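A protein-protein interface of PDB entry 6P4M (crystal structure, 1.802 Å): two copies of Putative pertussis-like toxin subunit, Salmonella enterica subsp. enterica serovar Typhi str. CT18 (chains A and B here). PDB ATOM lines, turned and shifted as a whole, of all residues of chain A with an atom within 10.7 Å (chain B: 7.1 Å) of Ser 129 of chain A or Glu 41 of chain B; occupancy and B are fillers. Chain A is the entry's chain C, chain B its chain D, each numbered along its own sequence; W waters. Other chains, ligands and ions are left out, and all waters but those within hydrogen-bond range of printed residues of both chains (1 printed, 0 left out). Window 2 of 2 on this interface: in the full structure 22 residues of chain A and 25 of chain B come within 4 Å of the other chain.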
ATOM      1  N   SER A  35       3.670 -27.100  -1.105  1.00  0.00           N
ATOM      2  CA  SER A  35       4.552 -25.951  -0.955  1.00  0.00           C
ATOM      3  C   SER A  35       5.509 -26.118   0.221  1.00  0.00           C
ATOM      4  O   SER A  35       5.317 -26.951   1.116  1.00  0.00           O
ATOM      5  CB  SER A  35       3.725 -24.668  -0.776  1.00  0.00           C
ATOM      6  OG  SER A  35       2.827 -24.487  -1.863  1.00  0.00           O
ATOM      7  N   ASP A  36       6.557 -25.291   0.212  1.00  0.00           N
ATOM      8  CA  ASP A  36       7.498 -25.217   1.324  1.00  0.00           C
ATOM      9  C   ASP A  36       8.164 -26.566   1.571  1.00  0.00           C
ATOM     10  O   ASP A  36       8.346 -26.981   2.716  1.00  0.00           O
ATOM     11  CB  ASP A  36       6.815 -24.716   2.601  1.00  0.00           C
ATOM     12  CG  ASP A  36       5.954 -23.489   2.362  1.00  0.00           C
ATOM     13  OD1 ASP A  36       6.377 -22.598   1.592  1.00  0.00           O
ATOM     14  OD2 ASP A  36       4.853 -23.418   2.949  1.00  0.00           O
ATOM     15  N   GLU A  37       8.523 -27.257   0.487  1.00  0.00           N
ATOM     16  CA  GLU A  37       9.190 -28.549   0.539  1.00  0.00           C
ATOM     17  C   GLU A  37      10.666 -28.405   0.188  1.00  0.00           C
ATOM     18  O   GLU A  37      11.078 -27.457  -0.480  1.00  0.00           O
ATOM     19  CB  GLU A  37       8.540 -29.538  -0.434  1.00  0.00           C
ATOM     20  CG  GLU A  37       7.022 -29.704  -0.261  1.00  0.00           C
ATOM     21  CD  GLU A  37       6.646 -30.849   0.663  1.00  0.00           C
ATOM     22  OE1 GLU A  37       7.484 -31.732   0.921  1.00  0.00           O
ATOM     23  OE2 GLU A  37       5.495 -30.861   1.135  1.00  0.00           O
ATOM     24  N   ALA A  60      10.033 -28.238   4.635  1.00  0.00           N
ATOM     25  CA  ALA A  60      11.221 -27.546   5.111  1.00  0.00           C
ATOM     26  C   ALA A  60      11.240 -27.450   6.630  1.00  0.00           C
ATOM     27  O   ALA A  60      12.309 -27.545   7.240  1.00  0.00           O
ATOM     28  CB  ALA A  60      11.310 -26.159   4.476  1.00  0.00           C
ATOM     29  N   GLN A  88      16.230 -29.427 -13.409  1.00  0.00           N
ATOM     30  CA  GLN A  88      15.755 -28.528 -12.362  1.00  0.00           C
ATOM     31  C   GLN A  88      15.684 -29.228 -11.016  1.00  0.00           C
ATOM     32  O   GLN A  88      15.939 -28.610  -9.977  1.00  0.00           O
ATOM     33  CB  GLN A  88      14.382 -27.954 -12.720  1.00  0.00           C
ATOM     34  CG  GLN A  88      14.052 -26.731 -11.871  1.00  0.00           C
ATOM     35  CD  GLN A  88      15.109 -25.675 -12.042  1.00  0.00           C
ATOM     36  OE1 GLN A  88      15.467 -25.337 -13.174  1.00  0.00           O
ATOM     37  NE2 GLN A  88      15.642 -25.162 -10.926  1.00  0.00           N
ATOM     38  N   TYR A  91      19.126 -29.153  -9.661  1.00  0.00           N
ATOM     39  CA  TYR A  91      19.545 -27.845  -9.168  1.00  0.00           C
ATOM     40  C   TYR A  91      18.947 -27.558  -7.793  1.00  0.00           C
ATOM     41  O   TYR A  91      19.659 -27.149  -6.870  1.00  0.00           O
ATOM     42  CB  TYR A  91      19.162 -26.739 -10.150  1.00  0.00           C
ATOM     43  CG  TYR A  91      19.589 -25.407  -9.590  1.00  0.00           C
ATOM     44  CD1 TYR A  91      20.939 -25.130  -9.404  1.00  0.00           C
ATOM     45  CD2 TYR A  91      18.655 -24.467  -9.157  1.00  0.00           C
ATOM     46  CE1 TYR A  91      21.360 -23.937  -8.855  1.00  0.00           C
ATOM     47  CE2 TYR A  91      19.066 -23.258  -8.597  1.00  0.00           C
ATOM     48  CZ  TYR A  91      20.430 -23.003  -8.457  1.00  0.00           C
ATOM     49  OH  TYR A  91      20.889 -21.825  -7.913  1.00  0.00           O
ATOM     50  N   PHE A  92      17.639 -27.784  -7.635  1.00  0.00           N
ATOM     51  CA  PHE A  92      16.997 -27.558  -6.343  1.00  0.00           C
ATOM     52  C   PHE A  92      17.463 -28.564  -5.288  1.00  0.00           C
ATOM     53  O   PHE A  92      17.499 -28.241  -4.092  1.00  0.00           O
ATOM     54  CB  PHE A  92      15.481 -27.621  -6.508  1.00  0.00           C
ATOM     55  CG  PHE A  92      14.868 -26.393  -7.154  1.00  0.00           C
ATOM     56  CD1 PHE A  92      15.478 -25.145  -7.063  1.00  0.00           C
ATOM     57  CD2 PHE A  92      13.658 -26.494  -7.839  1.00  0.00           C
ATOM     58  CE1 PHE A  92      14.884 -24.015  -7.655  1.00  0.00           C
ATOM     59  CE2 PHE A  92      13.063 -25.378  -8.436  1.00  0.00           C
ATOM     60  CZ  PHE A  92      13.677 -24.134  -8.338  1.00  0.00           C
ATOM     61  N   THR A  95      20.846 -27.097  -3.999  1.00  0.00           N
ATOM     62  CA  THR A  95      20.779 -25.948  -3.088  1.00  0.00           C
ATOM     63  C   THR A  95      20.051 -26.275  -1.792  1.00  0.00           C
ATOM     64  O   THR A  95      20.339 -25.668  -0.750  1.00  0.00           O
ATOM     65  CB  THR A  95      20.084 -24.756  -3.742  1.00  0.00           C
ATOM     66  OG1 THR A  95      18.712 -25.087  -4.000  1.00  0.00           O
ATOM     67  CG2 THR A  95      20.773 -24.345  -5.032  1.00  0.00           C
ATOM     68  N   GLY A  96      19.102 -27.203  -1.836  1.00  0.00           N
ATOM     69  CA  GLY A  96      18.293 -27.507  -0.673  1.00  0.00           C
ATOM     70  C   GLY A  96      17.299 -26.428  -0.317  1.00  0.00           C
ATOM     71  O   GLY A  96      16.785 -26.416   0.809  1.00  0.00           O
ATOM     72  N   GLN A  97      17.016 -25.521  -1.249  1.00  0.00           N
ATOM     73  CA  GLN A  97      16.073 -24.440  -1.008  1.00  0.00           C
ATOM     74  C   GLN A  97      14.640 -24.966  -0.986  1.00  0.00           C
ATOM     75  O   GLN A  97      14.328 -26.047  -1.498  1.00  0.00           O
ATOM     76  CB  GLN A  97      16.204 -23.351  -2.076  1.00  0.00           C
ATOM     77  CG  GLN A  97      15.749 -23.776  -3.473  1.00  0.00           C
ATOM     78  CD  GLN A  97      16.189 -22.798  -4.559  1.00  0.00           C
ATOM     79  OE1 GLN A  97      15.515 -21.797  -4.820  1.00  0.00           O
ATOM     80  NE2 GLN A  97      17.315 -23.091  -5.202  1.00  0.00           N
ATOM     81  N   SER A  98      13.764 -24.175  -0.375  1.00  0.00           N
ATOM     82  CA  SER A  98      12.351 -24.518  -0.320  1.00  0.00           C
ATOM     83  C   SER A  98      11.710 -24.360  -1.695  1.00  0.00           C
ATOM     84  O   SER A  98      11.997 -23.407  -2.424  1.00  0.00           O
ATOM     85  CB  SER A  98      11.650 -23.628   0.709  1.00  0.00           C
ATOM     86  OG  SER A  98      10.276 -23.944   0.799  1.00  0.00           O
ATOM     87  N   VAL A  99      10.848 -25.316  -2.067  1.00  0.00           N
ATOM     88  CA  VAL A  99      10.238 -25.351  -3.393  1.00  0.00           C
ATOM     89  C   VAL A  99       8.771 -25.755  -3.270  1.00  0.00           C
ATOM     90  O   VAL A  99       8.319 -26.235  -2.230  1.00  0.00           O
ATOM     91  CB  VAL A  99      10.957 -26.328  -4.349  1.00  0.00           C
ATOM     92  CG1 VAL A  99      12.411 -25.890  -4.577  1.00  0.00           C
ATOM     93  CG2 VAL A  99      10.906 -27.735  -3.798  1.00  0.00           C
ATOM     94  N   ARG A 100       8.034 -25.551  -4.356  1.00  0.00           N
ATOM     95  CA  ARG A 100       6.717 -26.150  -4.553  1.00  0.00           C
ATOM     96  C   ARG A 100       6.846 -27.236  -5.606  1.00  0.00           C
ATOM     97  O   ARG A 100       7.379 -26.997  -6.696  1.00  0.00           O
ATOM     98  CB  ARG A 100       5.671 -25.119  -4.989  1.00  0.00           C
ATOM     99  CG  ARG A 100       4.321 -25.730  -5.374  1.00  0.00           C
ATOM    100  CD  ARG A 100       3.316 -24.653  -5.751  1.00  0.00           C
ATOM    101  NE  ARG A 100       2.935 -23.864  -4.578  1.00  0.00           N
ATOM    102  CZ  ARG A 100       2.077 -22.850  -4.614  1.00  0.00           C
ATOM    103  NH1 ARG A 100       1.508 -22.513  -5.762  1.00  0.00           N
ATOM    104  NH2 ARG A 100       1.781 -22.184  -3.500  1.00  0.00           N
ATOM    105  N   LEU A 125       8.204 -27.662 -10.974  1.00  0.00           N
ATOM    106  CA  LEU A 125       8.968 -27.271  -9.792  1.00  0.00           C
ATOM    107  C   LEU A 125       9.045 -25.756  -9.748  1.00  0.00           C
ATOM    108  O   LEU A 125       9.370 -25.129 -10.757  1.00  0.00           O
ATOM    109  CB  LEU A 125      10.389 -27.859  -9.807  1.00  0.00           C
ATOM    110  CG  LEU A 125      10.452 -29.379  -9.652  1.00  0.00           C
ATOM    111  CD1 LEU A 125      11.836 -29.919 -10.061  1.00  0.00           C
ATOM    112  CD2 LEU A 125      10.099 -29.785  -8.227  1.00  0.00           C
ATOM    113  N   SER A 126       8.735 -25.176  -8.592  1.00  0.00           N
ATOM    114  CA  SER A 126       8.715 -23.725  -8.406  1.00  0.00           C
ATOM    115  C   SER A 126       9.579 -23.339  -7.216  1.00  0.00           C
ATOM    116  O   SER A 126       9.523 -23.992  -6.176  1.00  0.00           O
ATOM    117  CB  SER A 126       7.284 -23.222  -8.159  1.00  0.00           C
ATOM    118  OG  SER A 126       6.421 -23.689  -9.166  1.00  0.00           O
ATOM    119  N   SER A 127      10.357 -22.263  -7.349  1.00  0.00           N
ATOM    120  CA  SER A 127      11.055 -21.746  -6.179  1.00  0.00           C
ATOM    121  C   SER A 127      10.068 -21.115  -5.196  1.00  0.00           C
ATOM    122  O   SER A 127       8.982 -20.660  -5.571  1.00  0.00           O
ATOM    123  CB  SER A 127      12.105 -20.713  -6.586  1.00  0.00           C
ATOM    124  OG  SER A 127      11.484 -19.626  -7.238  1.00  0.00           O
ATOM    125  N   CYS A 128      10.459 -21.093  -3.923  1.00  0.00           N
ATOM    126  CA  CYS A 128       9.703 -20.445  -2.858  1.00  0.00           C
ATOM    127  C   CYS A 128      10.545 -19.402  -2.151  1.00  0.00           C
ATOM    128  O   CYS A 128      10.555 -19.315  -0.925  1.00  0.00           O
ATOM    129  CB  CYS A 128       9.201 -21.452  -1.841  1.00  0.00           C
ATOM    130  SG  CYS A 128       8.257 -22.662  -2.641  1.00  0.00           S
ATOM    131  N   SER A 129      11.285 -18.614  -2.918  1.00  0.00           N
ATOM    132  CA  SER A 129      12.015 -17.523  -2.302  1.00  0.00           C
ATOM    133  C   SER A 129      11.031 -16.464  -1.844  1.00  0.00           C
ATOM    134  O   SER A 129      10.062 -16.157  -2.542  1.00  0.00           O
ATOM    135  CB  SER A 129      13.016 -16.918  -3.274  1.00  0.00           C
ATOM    136  OG  SER A 129      13.304 -15.573  -2.945  1.00  0.00           O
ATOM    137  N   ALA A 130      11.262 -15.950  -0.645  1.00  0.00           N
ATOM    138  CA  ALA A 130      10.544 -14.770  -0.163  1.00  0.00           C
ATOM    139  C   ALA A 130       9.032 -15.040  -0.180  1.00  0.00           C
ATOM    140  O   ALA A 130       8.604 -16.180   0.030  1.00  0.00           O
ATOM    141  CB  ALA A 130      10.971 -13.563  -0.983  1.00  0.00           C
ATOM    142  N   THR A 131       8.269 -13.992  -0.479  1.00  0.00           N
ATOM    143  CA  THR A 131       6.808 -13.883  -0.446  1.00  0.00           C
ATOM    144  C   THR A 131       6.020 -15.192  -0.422  1.00  0.00           C
ATOM    145  O   THR A 131       5.335 -15.492   0.557  1.00  0.00           O
ATOM    146  CB  THR A 131       6.349 -13.059  -1.652  1.00  0.00           C
ATOM    147  OG1 THR A 131       7.057 -13.484  -2.825  1.00  0.00           O
ATOM    148  CG2 THR A 131       6.625 -11.583  -1.416  1.00  0.00           C
ATOM    149  N   GLN A 132       6.069 -15.940  -1.517  1.00  0.00           N
ATOM    150  CA  GLN A 132       5.289 -17.163  -1.647  1.00  0.00           C
ATOM    151  C   GLN A 132       5.911 -17.982  -2.770  1.00  0.00           C
ATOM    152  O   GLN A 132       7.014 -17.669  -3.231  1.00  0.00           O
ATOM    153  CB  GLN A 132       3.811 -16.831  -1.908  1.00  0.00           C
ATOM    154  CG  GLN A 132       3.597 -16.089  -3.213  1.00  0.00           C
ATOM    155  CD  GLN A 132       2.134 -15.784  -3.489  1.00  0.00           C
ATOM    156  OE1 GLN A 132       1.273 -16.671  -3.466  1.00  0.00           O
ATOM    157  NE2 GLN A 132       1.847 -14.516  -3.754  1.00  0.00           N
ATOM    158  N   CYS A 133       5.211 -19.018  -3.219  1.00  0.00           N
ATOM    159  CA  CYS A 133       5.750 -19.890  -4.250  1.00  0.00           C
ATOM    160  C   CYS A 133       5.480 -19.300  -5.623  1.00  0.00           C
ATOM    161  O   CYS A 133       4.373 -18.822  -5.905  1.00  0.00           O
ATOM    162  CB  CYS A 133       5.160 -21.290  -4.145  1.00  0.00           C
ATOM    163  SG  CYS A 133       5.338 -21.951  -2.487  1.00  0.00           S
ATOM    164  N   PHE A 134       6.500 -19.336  -6.476  1.00  0.00           N
ATOM    165  CA  PHE A 134       6.409 -18.743  -7.804  1.00  0.00           C
ATOM    166  C   PHE A 134       5.919 -19.801  -8.792  1.00  0.00           C
ATOM    167  O   PHE A 134       6.659 -20.348  -9.608  1.00  0.00           O
ATOM    168  CB  PHE A 134       7.758 -18.167  -8.215  1.00  0.00           C
ATOM    169  CG  PHE A 134       7.755 -17.512  -9.567  1.00  0.00           C
ATOM    170  CD1 PHE A 134       6.975 -16.393  -9.811  1.00  0.00           C
ATOM    171  CD2 PHE A 134       8.556 -18.004 -10.586  1.00  0.00           C
ATOM    172  CE1 PHE A 134       6.982 -15.785 -11.044  1.00  0.00           C
ATOM    173  CE2 PHE A 134       8.572 -17.402 -11.830  1.00  0.00           C
ATOM    174  CZ  PHE A 134       7.785 -16.289 -12.067  1.00  0.00           C
ATOM    175  N   GLY A 135       4.634 -20.098  -8.706  1.00  0.00           N
ATOM    176  CA  GLY A 135       4.050 -21.053  -9.621  1.00  0.00           C
ATOM    177  C   GLY A 135       2.549 -21.115  -9.448  1.00  0.00           C
ATOM    178  O   GLY A 135       1.992 -20.495  -8.533  1.00  0.00           O
ATOM    179  N   PRO A 136       1.869 -21.865 -10.316  1.00  0.00           N
ATOM    180  CA  PRO A 136       0.403 -21.863 -10.295  1.00  0.00           C
ATOM    181  C   PRO A 136      -0.122 -22.279  -8.942  1.00  0.00           C
ATOM    182  O   PRO A 136       0.365 -23.233  -8.320  1.00  0.00           O
ATOM    183  CB  PRO A 136       0.019 -22.865 -11.392  1.00  0.00           C
ATOM    184  CG  PRO A 136       1.205 -23.723 -11.552  1.00  0.00           C
ATOM    185  CD  PRO A 136       2.392 -22.808 -11.315  1.00  0.00           C
ATOM    186  N   LYS A 137      -1.138 -21.539  -8.512  1.00  0.00           N
ATOM    187  CA  LYS A 137      -1.631 -21.516  -7.164  1.00  0.00           C
ATOM    188  C   LYS A 137      -3.155 -21.631  -7.224  1.00  0.00           C
ATOM    189  O   LYS A 137      -3.721 -21.970  -8.275  1.00  0.00           O
ATOM    190  CB  LYS A 137      -1.195 -20.215  -6.479  1.00  0.00           C
ATOM    191  CG  LYS A 137      -1.188 -19.022  -7.434  1.00  0.00           C
ATOM    192  CD  LYS A 137      -0.138 -17.990  -7.052  1.00  0.00           C
ATOM    193  CE  LYS A 137       0.188 -17.093  -8.230  1.00  0.00           C
ATOM    194  NZ  LYS A 137       1.488 -16.373  -8.033  1.00  0.00           N
ATOM    195  N   VAL B  38      17.648  -8.443 -10.445  1.00  0.00           N
ATOM    196  CA  VAL B  38      18.150  -9.679  -9.854  1.00  0.00           C
ATOM    197  C   VAL B  38      17.094 -10.753 -10.061  1.00  0.00           C
ATOM    198  O   VAL B  38      15.917 -10.529  -9.766  1.00  0.00           O
ATOM    199  CB  VAL B  38      18.483  -9.495  -8.363  1.00  0.00           C
ATOM    200  CG1 VAL B  38      18.842 -10.823  -7.708  1.00  0.00           C
ATOM    201  CG2 VAL B  38      19.638  -8.482  -8.208  1.00  0.00           C
ATOM    202  N   ILE B  39      17.497 -11.901 -10.603  1.00  0.00           N
ATOM    203  CA  ILE B  39      16.535 -12.986 -10.782  1.00  0.00           C
ATOM    204  C   ILE B  39      16.229 -13.585  -9.415  1.00  0.00           C
ATOM    205  O   ILE B  39      17.117 -14.110  -8.735  1.00  0.00           O
ATOM    206  CB  ILE B  39      17.066 -14.039 -11.763  1.00  0.00           C
ATOM    207  CG1 ILE B  39      17.351 -13.407 -13.122  1.00  0.00           C
ATOM    208  CG2 ILE B  39      16.060 -15.199 -11.936  1.00  0.00           C
ATOM    209  CD1 ILE B  39      17.752 -14.435 -14.181  1.00  0.00           C
ATOM    210  N   SER B  40      14.964 -13.501  -8.992  1.00  0.00           N
ATOM    211  CA  SER B  40      14.618 -13.870  -7.626  1.00  0.00           C
ATOM    212  C   SER B  40      13.756 -15.119  -7.521  1.00  0.00           C
ATOM    213  O   SER B  40      13.643 -15.675  -6.422  1.00  0.00           O
ATOM    214  CB  SER B  40      13.908 -12.704  -6.924  1.00  0.00           C
ATOM    215  OG  SER B  40      12.598 -12.542  -7.417  1.00  0.00           O
ATOM    216  N   GLU B  41      13.156 -15.577  -8.619  1.00  0.00           N
ATOM    217  CA  GLU B  41      12.374 -16.808  -8.632  1.00  0.00           C
ATOM    218  C   GLU B  41      12.553 -17.516  -9.964  1.00  0.00           C
ATOM    219  O   GLU B  41      12.814 -16.882 -10.988  1.00  0.00           O
ATOM    220  CB  GLU B  41      10.875 -16.568  -8.442  1.00  0.00           C
ATOM    221  CG  GLU B  41      10.503 -15.612  -7.348  1.00  0.00           C
ATOM    222  CD  GLU B  41      10.592 -16.236  -5.977  1.00  0.00           C
ATOM    223  OE1 GLU B  41      10.800 -17.470  -5.873  1.00  0.00           O
ATOM    224  OE2 GLU B  41      10.453 -15.487  -4.992  1.00  0.00           O
ATOM    225  N   LEU B  42      12.359 -18.835  -9.942  1.00  0.00           N
ATOM    226  CA  LEU B  42      12.454 -19.662 -11.137  1.00  0.00           C
ATOM    227  C   LEU B  42      11.443 -20.793 -11.041  1.00  0.00           C
ATOM    228  O   LEU B  42      11.327 -21.435  -9.992  1.00  0.00           O
ATOM    229  CB  LEU B  42      13.871 -20.236 -11.301  1.00  0.00           C
ATOM    230  CG  LEU B  42      14.114 -21.306 -12.366  1.00  0.00           C
ATOM    231  CD1 LEU B  42      13.867 -20.753 -13.748  1.00  0.00           C
ATOM    232  CD2 LEU B  42      15.546 -21.821 -12.242  1.00  0.00           C
ATOM    233  N   HIS B  43      10.731 -21.045 -12.142  1.00  0.00           N
ATOM    234  CA  HIS B  43       9.717 -22.095 -12.219  1.00  0.00           C
ATOM    235  C   HIS B  43       9.883 -22.851 -13.527  1.00  0.00           C
ATOM    236  O   HIS B  43      10.146 -22.240 -14.563  1.00  0.00           O
ATOM    237  CB  HIS B  43       8.289 -21.499 -12.135  1.00  0.00           C
ATOM    238  CG  HIS B  43       7.206 -22.418 -12.624  1.00  0.00           C
ATOM    239  ND1 HIS B  43       6.474 -23.222 -11.777  1.00  0.00           N
ATOM    240  CD2 HIS B  43       6.715 -22.638 -13.865  1.00  0.00           C
ATOM    241  CE1 HIS B  43       5.585 -23.906 -12.478  1.00  0.00           C
ATOM    242  NE2 HIS B  43       5.711 -23.571 -13.748  1.00  0.00           N
ATOM    243  N   CYS B  54       9.700 -19.892 -16.316  1.00  0.00           N
ATOM    244  CA  CYS B  54       9.408 -18.505 -15.996  1.00  0.00           C
ATOM    245  C   CYS B  54      10.396 -18.021 -14.954  1.00  0.00           C
ATOM    246  O   CYS B  54      10.852 -18.794 -14.114  1.00  0.00           O
ATOM    247  CB  CYS B  54       7.993 -18.347 -15.454  1.00  0.00           C
ATOM    248  SG  CYS B  54       6.740 -18.887 -16.627  1.00  0.00           S
ATOM    249  N   ILE B  55      10.704 -16.725 -14.996  1.00  0.00           N
ATOM    250  CA  ILE B  55      11.525 -16.101 -13.968  1.00  0.00           C
ATOM    251  C   ILE B  55      10.812 -14.857 -13.468  1.00  0.00           C
ATOM    252  O   ILE B  55      10.010 -14.245 -14.182  1.00  0.00           O
ATOM    253  CB  ILE B  55      12.946 -15.731 -14.461  1.00  0.00           C
ATOM    254  CG1 ILE B  55      12.886 -14.919 -15.749  1.00  0.00           C
ATOM    255  CG2 ILE B  55      13.782 -16.990 -14.693  1.00  0.00           C
ATOM    256  CD1 ILE B  55      14.250 -14.323 -16.137  1.00  0.00           C
ATOM    257  N   LYS B  56      11.114 -14.490 -12.230  1.00  0.00           N
ATOM    258  CA  LYS B  56      10.703 -13.217 -11.658  1.00  0.00           C
ATOM    259  C   LYS B  56      11.971 -12.459 -11.316  1.00  0.00           C
ATOM    260  O   LYS B  56      12.904 -13.045 -10.759  1.00  0.00           O
ATOM    261  CB  LYS B  56       9.852 -13.422 -10.414  1.00  0.00           C
ATOM    262  CG  LYS B  56       9.325 -12.133  -9.753  1.00  0.00           C
ATOM    263  CD  LYS B  56       8.434 -12.543  -8.569  1.00  0.00           C
ATOM    264  CE  LYS B  56       8.026 -11.373  -7.687  1.00  0.00           C
ATOM    265  NZ  LYS B  56       7.201 -11.847  -6.529  1.00  0.00           N
ATOM    266  N   THR B  57      12.020 -11.175 -11.665  1.00  0.00           N
ATOM    267  CA  THR B  57      13.169 -10.343 -11.331  1.00  0.00           C
ATOM    268  C   THR B  57      12.699  -9.096 -10.596  1.00  0.00           C
ATOM    269  O   THR B  57      11.563  -8.643 -10.768  1.00  0.00           O
ATOM    270  CB  THR B  57      14.000  -9.937 -12.579  1.00  0.00           C
ATOM    271  OG1 THR B  57      13.325  -8.913 -13.326  1.00  0.00           O
ATOM    272  CG2 THR B  57      14.253 -11.142 -13.498  1.00  0.00           C
ATOM    273  N   TYR B  93      20.499 -16.688 -11.843  1.00  0.00           N
ATOM    274  CA  TYR B  93      19.744 -16.956 -10.624  1.00  0.00           C
ATOM    275  C   TYR B  93      20.664 -17.460  -9.521  1.00  0.00           C
ATOM    276  O   TYR B  93      20.550 -17.048  -8.363  1.00  0.00           O
ATOM    277  CB  TYR B  93      18.650 -17.981 -10.941  1.00  0.00           C
ATOM    278  CG  TYR B  93      17.741 -18.430  -9.818  1.00  0.00           C
ATOM    279  CD1 TYR B  93      17.059 -17.521  -9.020  1.00  0.00           C
ATOM    280  CD2 TYR B  93      17.517 -19.788  -9.605  1.00  0.00           C
ATOM    281  CE1 TYR B  93      16.199 -17.958  -8.030  1.00  0.00           C
ATOM    282  CE2 TYR B  93      16.667 -20.228  -8.615  1.00  0.00           C
ATOM    283  CZ  TYR B  93      16.011 -19.317  -7.832  1.00  0.00           C
ATOM    284  OH  TYR B  93      15.159 -19.786  -6.847  1.00  0.00           O
HETATM  285  O   HOH W   1       7.158 -15.675  -5.833  1.00  0.00           O
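Gln 88 of chain A touches Leu 42 of chain B (NE2 to CD2, 3.6 Å). Tyr 91 of chain A touches Tyr 93 of chain B (CE2 to CE2, 3.9 Å). CZ of Phe 92 of chain A touches O of Leu 42 of chain B, 3.9 Å away. Leu 125 of chain A touches His 43 of chain B. OH of Tyr 93 of chain B touches CB of Ser 127 of chain A, 3.2 Å away. Phe 134 of chain A touches Glu 41 of chain B. O of Cys 54 of chain B touches CE2 of Phe 134 of chain A, 3.5 Å away. CE1 of Phe 134 of chain A touches CB of Lys 56 of chain B (3.8 Å). Gly 135 of chain A touches His 43 of chain B (CA to ND1, 3.9 Å). Pro 136 of chain A touches His 43 of chain B.
The backbone NH (N) of Ser 40 of chain B lies within hydrogen-bond range of the backbone carbonyl oxygen (O) of Lys 56 of chain B (2.8 Å). OG of Ser 126 of chain A sits close to O of Phe 134 of chain A (3.4 Å). The backbone carbonyl oxygen of Pro 136 of chain A sits at hydrogen-bond distance from the guanidinium group of Arg 100 of chain A (2.9 Å). The backbone NH (N) of Arg 100 of chain A sits at hydrogen-bond distance from the backbone carbonyl oxygen (O) of Ser 126 of chain A. O of Phe 92 of chain A lies within hydrogen-bond range of OG1 of Thr 95 of chain A, 3.4 Å away. The backbone NH of Phe 134 of chain A lies within hydrogen-bond range of the backbone carbonyl oxygen of Ser 127 of chain A (3.0 Å).
No position is printed for both chains.
Water W1 bridges the backbone carbonyl oxygen of Gln 132 of chain A (3.3 Å) and the side-chain carboxylate of Glu 41 of chain B (3.4 Å).
Of the 11 printed residues of chain B, 8 touch a printed residue of chain A. Hydrophobic or aromatic side chains of chain B that line the printed part of chain A: Leu 42, His 43 and Tyr 93.
Printed residues of chain B within 4 Å of Gln 88 of chain A: Leu 42. Printed residues of chain B within 4 Å of Tyr 91 of chain A: Tyr 93 (3.9 Å). Ser 129 of chain A touches two residues of chain B. No residue of chain B comes within 4 Å of Ala 130 of chain A. Of chain A, only Ser 127 (2.6 Å), Ser 129 (2.6 Å) and Phe 134 (3.4 Å) come within 4 Å of Glu 41 of chain B. Of chain A, only Phe 134 comes within 4 Å of Lys 56 of chain B. Of the printed residues of chain A, Tyr 93 of chain B touches Tyr 91 (3.9 Å), Gln 97 (2.9 Å) and Ser 127 (3.2 Å). The nearest residue of chain B that does not touch Ser 129 of chain A is Tyr 93 of chain B (5.1 Å).
The backbone NH (N) of Ser 127 of chain A sits at hydrogen-bond distance from the backbone carbonyl oxygen (O) of Leu 42 of chain B. The side-chain hydroxyl (OG) of Ser 126 of chain A is in hydrogen-bond range of a ring nitrogen (ND1) of His 43 of chain B (2.7 Å). The side-chain carboxylate (OE1) of Glu 41 of chain B lies within hydrogen-bond range of the backbone NH (N) of Ser 129 of chain A, 3.2 Å away. OE1 of Gln 97 of chain A lies within hydrogen-bond range of OH of Tyr 93 of chain B (2.9 Å). OG of Ser 127 of chain A is in hydrogen-bond range of OE1 of Glu 41 of chain B, 2.6 Å away. The backbone carbonyl oxygen (O) of Ser 40 of chain B sits close to the side-chain hydroxyl (OG) of Ser 129 of chain A, at 3.5 Å.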
